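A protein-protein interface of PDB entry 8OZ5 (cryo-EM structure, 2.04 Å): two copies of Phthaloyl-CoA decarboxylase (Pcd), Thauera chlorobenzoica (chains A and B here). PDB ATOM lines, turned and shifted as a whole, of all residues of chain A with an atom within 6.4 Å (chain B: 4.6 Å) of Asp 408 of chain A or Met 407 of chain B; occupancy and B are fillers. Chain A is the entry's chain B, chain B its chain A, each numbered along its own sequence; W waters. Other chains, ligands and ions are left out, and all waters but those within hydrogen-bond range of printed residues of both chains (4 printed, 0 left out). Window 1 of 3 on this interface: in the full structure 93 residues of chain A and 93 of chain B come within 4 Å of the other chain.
Water W4 bridges OD2 of Asp 408 of chain B and N of Cys 356 of chain A. Water W3 lies within hydrogen-bond range of the side-chain carboxylate of Asp 408 of chain A (2.6 Å) and the backbone NH of Cys 356 of chain B (3.1 Å). Water W2 lies within hydrogen-bond range of the backbone NH of Met 407 of chain B (2.7 Å) and the side-chain carboxylate of Asp 408 of chain A (3.3 Å). Water W1 lies within hydrogen-bond range of N of Met 407 of chain A (2.7 Å) and OD2 of Asp 408 of chain B (3.3 Å).
Among the printed residues, merely in contact across the chains: Cys 356 of chain A with Asp 408 of chain B, Cys 356 of chain A with Met 411 of chain B, Met 407 of chain A with Asp 408 of chain B, Asp 408 of chain A with Met 407 of chain B, Met 411 of chain A with Cys 356 of chain B, Met 411 of chain A with Met 411 of chain B, Trp 412 of chain A with Cys 356 of chain B and Trp 505 of chain A with Cys 356 of chain B.
SG of Cys 356 of chain A lies close to SD of Met 407 of chain A, at 3.6 Å. The side-chain sulfur (SG) of Cys 356 of chain B sits close to the side-chain sulfur (SD) of Met 407 of chain B, at 3.6 Å. The side-chain carboxylate (OD1) of Asp 409 of chain A lies within hydrogen-bond range of the indole nitrogen (NE1) of Trp 505 of chain A (3.4 Å).
Of the 11 printed residues of chain A, 6 touch a printed residue of chain B. Printed residues of chain A that touch a printed residue of chain B: Cys 356, Met 407, Asp 408, Met 411, Trp 412 and Trp 505. Along chain A the printed residues that touch a printed residue of chain B span positions 356 to 505. Of the 11 printed residues of chain B, 4 touch a printed residue of chain A. Printed residues of chain B that touch a printed residue of chain A: Cys 356, Met 407, Asp 408 and Met 411. Among the printed residues, 9 pairs touch across the chains. Among the printed residues, no Asp or Glu carboxylate lies within 4 Å of a Lys or Arg side-chain nitrogen of the other chain.
O of Asp 408 of chain A lies close to SG of Cys 356 of chain B (3.8 Å).
Cys 356 of chain A touches Asp 408 of chain B, and with the chains exchanged Asp 408 of chain A touches Cys 356 of chain B. Cys 356 of chain A touches Met 411 of chain B, and with the chains exchanged Met 411 of chain A touches Cys 356 of chain B. Met 407 of chain A touches Asp 408 of chain B, and with the chains exchanged Asp 408 of chain A touches Met 407 of chain B. Met 411 of chain B touches its own counterpart, Met 411 of chain A. 7 positions are printed for both chains. Of the 9 pairs that touch across the chains among the printed residues, 7 have their exchanged pair printed and touching as well.
Of the printed residues of chain B, Cys 356 of chain A touches Asp 408 and Met 411. Ser 406 of chain A touches none of the printed residues of chain B. Asp 408 of chain A touches two residues of chain B. Printed residues of chain B within 4 Å of Trp 412 of chain A: Cys 356 (3.2 Å). Of the printed residues of chain B, Trp 505 of chain A touches Cys 356. Ile 404 of chain B touches none of the printed residues of chain A. Printed residues of chain A within 4 Å of Met 407 of chain B: Asp 408 (3.3 Å). Of the printed residues of chain A, Asp 408 of chain B touches Cys 356 (3.1 Å) and Met 407 (3.2 Å). Printed residues of chain A within 4 Å of Met 411 of chain B: Cys 356 (3.7 Å) and Met 411 (3.3 Å). The nearest residue of chain A that does not touch Met 407 of chain B is Met 411 of chain A (4.1 Å). The nearest printed residue of chain A that does not touch Met 411 of chain B is Ile 410 of chain A (4.1 Å).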
ATOM      1  N   CYS A 356      -8.602  16.458   4.121  1.00  0.00           N
ATOM      2  CA  CYS A 356      -7.446  15.854   3.474  1.00  0.00           C
ATOM      3  C   CYS A 356      -6.937  14.604   4.175  1.00  0.00           C
ATOM      4  O   CYS A 356      -5.981  13.995   3.689  1.00  0.00           O
ATOM      5  CB  CYS A 356      -6.310  16.874   3.376  1.00  0.00           C
ATOM      6  SG  CYS A 356      -5.697  17.454   4.965  1.00  0.00           S
ATOM      7  N   SER A 406      -5.908  24.858   9.739  1.00  0.00           N
ATOM      8  CA  SER A 406      -5.072  25.233   8.608  1.00  0.00           C
ATOM      9  C   SER A 406      -4.025  24.151   8.389  1.00  0.00           C
ATOM     10  O   SER A 406      -3.200  23.897   9.271  1.00  0.00           O
ATOM     11  CB  SER A 406      -4.405  26.585   8.855  1.00  0.00           C
ATOM     12  OG  SER A 406      -3.669  27.008   7.722  1.00  0.00           O
ATOM     13  N   MET A 407      -4.061  23.511   7.220  1.00  0.00           N
ATOM     14  CA  MET A 407      -3.051  22.506   6.920  1.00  0.00           C
ATOM     15  C   MET A 407      -1.676  23.126   6.729  1.00  0.00           C
ATOM     16  O   MET A 407      -0.663  22.462   6.969  1.00  0.00           O
ATOM     17  CB  MET A 407      -3.448  21.707   5.680  1.00  0.00           C
ATOM     18  CG  MET A 407      -4.542  20.688   5.932  1.00  0.00           C
ATOM     19  SD  MET A 407      -4.245  19.701   7.407  1.00  0.00           S
ATOM     20  CE  MET A 407      -5.233  20.591   8.602  1.00  0.00           C
ATOM     21  N   ASP A 408      -1.617  24.390   6.309  1.00  0.00           N
ATOM     22  CA  ASP A 408      -0.332  25.075   6.229  1.00  0.00           C
ATOM     23  C   ASP A 408       0.285  25.238   7.609  1.00  0.00           C
ATOM     24  O   ASP A 408       1.497  25.068   7.780  1.00  0.00           O
ATOM     25  CB  ASP A 408      -0.500  26.436   5.558  1.00  0.00           C
ATOM     26  CG  ASP A 408      -1.059  26.326   4.161  1.00  0.00           C
ATOM     27  OD1 ASP A 408      -2.257  26.011   4.027  1.00  0.00           O
ATOM     28  OD2 ASP A 408      -0.304  26.556   3.197  1.00  0.00           O
ATOM     29  N   ASP A 409      -0.533  25.554   8.611  1.00  0.00           N
ATOM     30  CA  ASP A 409      -0.006  25.736   9.957  1.00  0.00           C
ATOM     31  C   ASP A 409       0.450  24.402  10.542  1.00  0.00           C
ATOM     32  O   ASP A 409       1.462  24.333  11.251  1.00  0.00           O
ATOM     33  CB  ASP A 409      -1.072  26.399  10.826  1.00  0.00           C
ATOM     34  CG  ASP A 409      -0.496  27.073  12.044  1.00  0.00           C
ATOM     35  OD1 ASP A 409       0.107  28.154  11.891  1.00  0.00           O
ATOM     36  OD2 ASP A 409      -0.658  26.542  13.154  1.00  0.00           O
ATOM     37  N   ILE A 410      -0.264  23.322  10.214  1.00  0.00           N
ATOM     38  CA  ILE A 410       0.160  21.986  10.620  1.00  0.00           C
ATOM     39  C   ILE A 410       1.476  21.616   9.953  1.00  0.00           C
ATOM     40  O   ILE A 410       2.358  21.017  10.579  1.00  0.00           O
ATOM     41  CB  ILE A 410      -0.938  20.955  10.302  1.00  0.00           C
ATOM     42  CG1 ILE A 410      -2.229  21.296  11.043  1.00  0.00           C
ATOM     43  CG2 ILE A 410      -0.476  19.557  10.660  1.00  0.00           C
ATOM     44  CD1 ILE A 410      -2.051  21.458  12.527  1.00  0.00           C
ATOM     45  N   MET A 411       1.627  21.946   8.669  1.00  0.00           N
ATOM     46  CA  MET A 411       2.891  21.687   7.988  1.00  0.00           C
ATOM     47  C   MET A 411       4.027  22.495   8.598  1.00  0.00           C
ATOM     48  O   MET A 411       5.154  22.002   8.698  1.00  0.00           O
ATOM     49  CB  MET A 411       2.757  21.996   6.498  1.00  0.00           C
ATOM     50  CG  MET A 411       3.921  21.509   5.655  1.00  0.00           C
ATOM     51  SD  MET A 411       4.001  19.714   5.536  1.00  0.00           S
ATOM     52  CE  MET A 411       2.297  19.331   5.146  1.00  0.00           C
ATOM     53  N   TRP A 412       3.747  23.728   9.017  1.00  0.00           N
ATOM     54  CA  TRP A 412       4.759  24.518   9.709  1.00  0.00           C
ATOM     55  C   TRP A 412       5.173  23.854  11.017  1.00  0.00           C
ATOM     56  O   TRP A 412       6.365  23.799  11.345  1.00  0.00           O
ATOM     57  CB  TRP A 412       4.231  25.929   9.963  1.00  0.00           C
ATOM     58  CG  TRP A 412       5.146  26.768  10.783  1.00  0.00           C
ATOM     59  CD1 TRP A 412       6.225  27.468  10.343  1.00  0.00           C
ATOM     60  CD2 TRP A 412       5.068  26.993  12.192  1.00  0.00           C
ATOM     61  NE1 TRP A 412       6.827  28.117  11.390  1.00  0.00           N
ATOM     62  CE2 TRP A 412       6.134  27.840  12.538  1.00  0.00           C
ATOM     63  CE3 TRP A 412       4.201  26.558  13.196  1.00  0.00           C
ATOM     64  CZ2 TRP A 412       6.356  28.264  13.843  1.00  0.00           C
ATOM     65  CZ3 TRP A 412       4.422  26.978  14.489  1.00  0.00           C
ATOM     66  CH2 TRP A 412       5.491  27.822  14.802  1.00  0.00           C
ATOM     67  N   CYS A 413       4.200  23.347  11.776  1.00  0.00           N
ATOM     68  CA  CYS A 413       4.515  22.628  13.007  1.00  0.00           C
ATOM     69  C   CYS A 413       5.351  21.388  12.720  1.00  0.00           C
ATOM     70  O   CYS A 413       6.287  21.070  13.461  1.00  0.00           O
ATOM     71  CB  CYS A 413       3.230  22.251  13.739  1.00  0.00           C
ATOM     72  SG  CYS A 413       2.224  23.654  14.228  1.00  0.00           S
ATOM     73  N   GLY A 504      -5.558  31.548   1.623  1.00  0.00           N
ATOM     74  CA  GLY A 504      -4.720  30.493   2.158  1.00  0.00           C
ATOM     75  C   GLY A 504      -4.198  30.742   3.558  1.00  0.00           C
ATOM     76  O   GLY A 504      -4.942  31.180   4.438  1.00  0.00           O
ATOM     77  N   TRP A 505      -2.911  30.457   3.771  1.00  0.00           N
ATOM     78  CA  TRP A 505      -2.324  30.613   5.098  1.00  0.00           C
ATOM     79  C   TRP A 505      -2.296  32.068   5.538  1.00  0.00           C
ATOM     80  O   TRP A 505      -2.295  32.351   6.741  1.00  0.00           O
ATOM     81  CB  TRP A 505      -0.911  30.035   5.117  1.00  0.00           C
ATOM     82  CG  TRP A 505      -0.407  29.735   6.487  1.00  0.00           C
ATOM     83  CD1 TRP A 505      -1.144  29.352   7.564  1.00  0.00           C
ATOM     84  CD2 TRP A 505       0.951  29.801   6.932  1.00  0.00           C
ATOM     85  NE1 TRP A 505      -0.332  29.169   8.653  1.00  0.00           N
ATOM     86  CE2 TRP A 505       0.961  29.440   8.291  1.00  0.00           C
ATOM     87  CE3 TRP A 505       2.159  30.129   6.315  1.00  0.00           C
ATOM     88  CZ2 TRP A 505       2.131  29.396   9.042  1.00  0.00           C
ATOM     89  CZ3 TRP A 505       3.318  30.087   7.061  1.00  0.00           C
ATOM     90  CH2 TRP A 505       3.297  29.722   8.410  1.00  0.00           C
ATOM     91  N   PRO B 354       6.730  25.901  -0.046  1.00  0.00           N
ATOM     92  CA  PRO B 354       5.576  26.694   0.379  1.00  0.00           C
ATOM     93  C   PRO B 354       5.934  27.660   1.497  1.00  0.00           C
ATOM     94  O   PRO B 354       6.947  27.522   2.183  1.00  0.00           O
ATOM     95  CB  PRO B 354       4.578  25.638   0.864  1.00  0.00           C
ATOM     96  CG  PRO B 354       5.413  24.476   1.230  1.00  0.00           C
ATOM     97  CD  PRO B 354       6.579  24.479   0.295  1.00  0.00           C
ATOM     98  N   CYS B 356       4.548  27.955   4.299  1.00  0.00           N
ATOM     99  CA  CYS B 356       4.489  27.296   5.596  1.00  0.00           C
ATOM    100  C   CYS B 356       5.748  26.514   5.941  1.00  0.00           C
ATOM    101  O   CYS B 356       5.816  25.943   7.033  1.00  0.00           O
ATOM    102  CB  CYS B 356       3.283  26.358   5.651  1.00  0.00           C
ATOM    103  SG  CYS B 356       3.332  25.015   4.454  1.00  0.00           S
ATOM    104  N   ILE B 364       9.325  20.654  -1.324  1.00  0.00           N
ATOM    105  CA  ILE B 364       8.536  19.585  -1.917  1.00  0.00           C
ATOM    106  C   ILE B 364       8.991  19.399  -3.355  1.00  0.00           C
ATOM    107  O   ILE B 364       9.057  20.367  -4.119  1.00  0.00           O
ATOM    108  CB  ILE B 364       7.026  19.885  -1.866  1.00  0.00           C
ATOM    109  CG1 ILE B 364       6.579  20.098  -0.423  1.00  0.00           C
ATOM    110  CG2 ILE B 364       6.242  18.755  -2.499  1.00  0.00           C
ATOM    111  CD1 ILE B 364       5.244  20.771  -0.296  1.00  0.00           C
ATOM    112  N   ILE B 404       1.096  20.128  -6.061  1.00  0.00           N
ATOM    113  CA  ILE B 404       2.234  20.472  -5.220  1.00  0.00           C
ATOM    114  C   ILE B 404       2.016  21.771  -4.457  1.00  0.00           C
ATOM    115  O   ILE B 404       2.719  22.029  -3.475  1.00  0.00           O
ATOM    116  CB  ILE B 404       3.515  20.553  -6.071  1.00  0.00           C
ATOM    117  CG1 ILE B 404       4.753  20.532  -5.179  1.00  0.00           C
ATOM    118  CG2 ILE B 404       3.512  21.804  -6.917  1.00  0.00           C
ATOM    119  CD1 ILE B 404       6.043  20.364  -5.939  1.00  0.00           C
ATOM    120  N   TYR B 405       1.059  22.596  -4.871  1.00  0.00           N
ATOM    121  CA  TYR B 405       0.827  23.884  -4.235  1.00  0.00           C
ATOM    122  C   TYR B 405      -0.231  23.836  -3.143  1.00  0.00           C
ATOM    123  O   TYR B 405      -0.466  24.855  -2.487  1.00  0.00           O
ATOM    124  CB  TYR B 405       0.422  24.920  -5.284  1.00  0.00           C
ATOM    125  CG  TYR B 405       1.394  25.010  -6.432  1.00  0.00           C
ATOM    126  CD1 TYR B 405       2.647  25.572  -6.257  1.00  0.00           C
ATOM    127  CD2 TYR B 405       1.062  24.528  -7.687  1.00  0.00           C
ATOM    128  CE1 TYR B 405       3.540  25.655  -7.299  1.00  0.00           C
ATOM    129  CE2 TYR B 405       1.949  24.606  -8.735  1.00  0.00           C
ATOM    130  CZ  TYR B 405       3.187  25.171  -8.536  1.00  0.00           C
ATOM    131  OH  TYR B 405       4.078  25.253  -9.577  1.00  0.00           O
ATOM    132  N   SER B 406      -0.871  22.693  -2.934  1.00  0.00           N
ATOM    133  CA  SER B 406      -1.905  22.545  -1.921  1.00  0.00           C
ATOM    134  C   SER B 406      -1.334  21.767  -0.745  1.00  0.00           C
ATOM    135  O   SER B 406      -0.933  20.609  -0.901  1.00  0.00           O
ATOM    136  CB  SER B 406      -3.128  21.832  -2.497  1.00  0.00           C
ATOM    137  OG  SER B 406      -4.178  21.770  -1.550  1.00  0.00           O
ATOM    138  N   MET B 407      -1.292  22.398   0.428  1.00  0.00           N
ATOM    139  CA  MET B 407      -0.814  21.691   1.608  1.00  0.00           C
ATOM    140  C   MET B 407      -1.779  20.599   2.041  1.00  0.00           C
ATOM    141  O   MET B 407      -1.356  19.612   2.650  1.00  0.00           O
ATOM    142  CB  MET B 407      -0.577  22.672   2.755  1.00  0.00           C
ATOM    143  CG  MET B 407       0.688  23.497   2.604  1.00  0.00           C
ATOM    144  SD  MET B 407       2.115  22.500   2.149  1.00  0.00           S
ATOM    145  CE  MET B 407       2.127  22.734   0.377  1.00  0.00           C
ATOM    146  N   ASP B 408      -3.067  20.749   1.734  1.00  0.00           N
ATOM    147  CA  ASP B 408      -4.015  19.677   2.011  1.00  0.00           C
ATOM    148  C   ASP B 408      -3.699  18.441   1.184  1.00  0.00           C
ATOM    149  O   ASP B 408      -3.783  17.313   1.681  1.00  0.00           O
ATOM    150  CB  ASP B 408      -5.441  20.148   1.740  1.00  0.00           C
ATOM    151  CG  ASP B 408      -5.825  21.343   2.579  1.00  0.00           C
ATOM    152  OD1 ASP B 408      -5.311  22.444   2.310  1.00  0.00           O
ATOM    153  OD2 ASP B 408      -6.640  21.181   3.508  1.00  0.00           O
ATOM    154  N   ASP B 409      -3.321  18.633  -0.079  1.00  0.00           N
ATOM    155  CA  ASP B 409      -3.015  17.493  -0.932  1.00  0.00           C
ATOM    156  C   ASP B 409      -1.723  16.816  -0.483  1.00  0.00           C
ATOM    157  O   ASP B 409      -1.604  15.584  -0.523  1.00  0.00           O
ATOM    158  CB  ASP B 409      -2.932  17.961  -2.383  1.00  0.00           C
ATOM    159  CG  ASP B 409      -3.118  16.840  -3.371  1.00  0.00           C
ATOM    160  OD1 ASP B 409      -4.267  16.388  -3.541  1.00  0.00           O
ATOM    161  OD2 ASP B 409      -2.129  16.419  -3.991  1.00  0.00           O
ATOM    162  N   ILE B 410      -0.760  17.608  -0.007  1.00  0.00           N
ATOM    163  CA  ILE B 410       0.464  17.051   0.561  1.00  0.00           C
ATOM    164  C   ILE B 410       0.155  16.261   1.825  1.00  0.00           C
ATOM    165  O   ILE B 410       0.727  15.189   2.058  1.00  0.00           O
ATOM    166  CB  ILE B 410       1.486  18.167   0.836  1.00  0.00           C
ATOM    167  CG1 ILE B 410       1.846  18.898  -0.457  1.00  0.00           C
ATOM    168  CG2 ILE B 410       2.732  17.602   1.488  1.00  0.00           C
ATOM    169  CD1 ILE B 410       2.319  17.988  -1.554  1.00  0.00           C
ATOM    170  N   MET B 411      -0.736  16.780   2.671  1.00  0.00           N
ATOM    171  CA  MET B 411      -1.132  16.041   3.865  1.00  0.00           C
ATOM    172  C   MET B 411      -1.843  14.745   3.505  1.00  0.00           C
ATOM    173  O   MET B 411      -1.658  13.728   4.181  1.00  0.00           O
ATOM    174  CB  MET B 411      -2.024  16.911   4.748  1.00  0.00           C
ATOM    175  CG  MET B 411      -2.272  16.343   6.133  1.00  0.00           C
ATOM    176  SD  MET B 411      -0.800  16.354   7.171  1.00  0.00           S
ATOM    177  CE  MET B 411      -0.215  18.022   6.900  1.00  0.00           C
HETATM  178  O   HOH W   1      -5.921  23.912   5.273  1.00  0.00           O
HETATM  179  O   HOH W   2      -2.083  24.955   0.870  1.00  0.00           O
HETATM  180  O   HOH W   3       1.978  27.773   2.665  1.00  0.00           O
HETATM  181  O   HOH W   4      -8.512  19.502   4.273  1.00  0.00           O
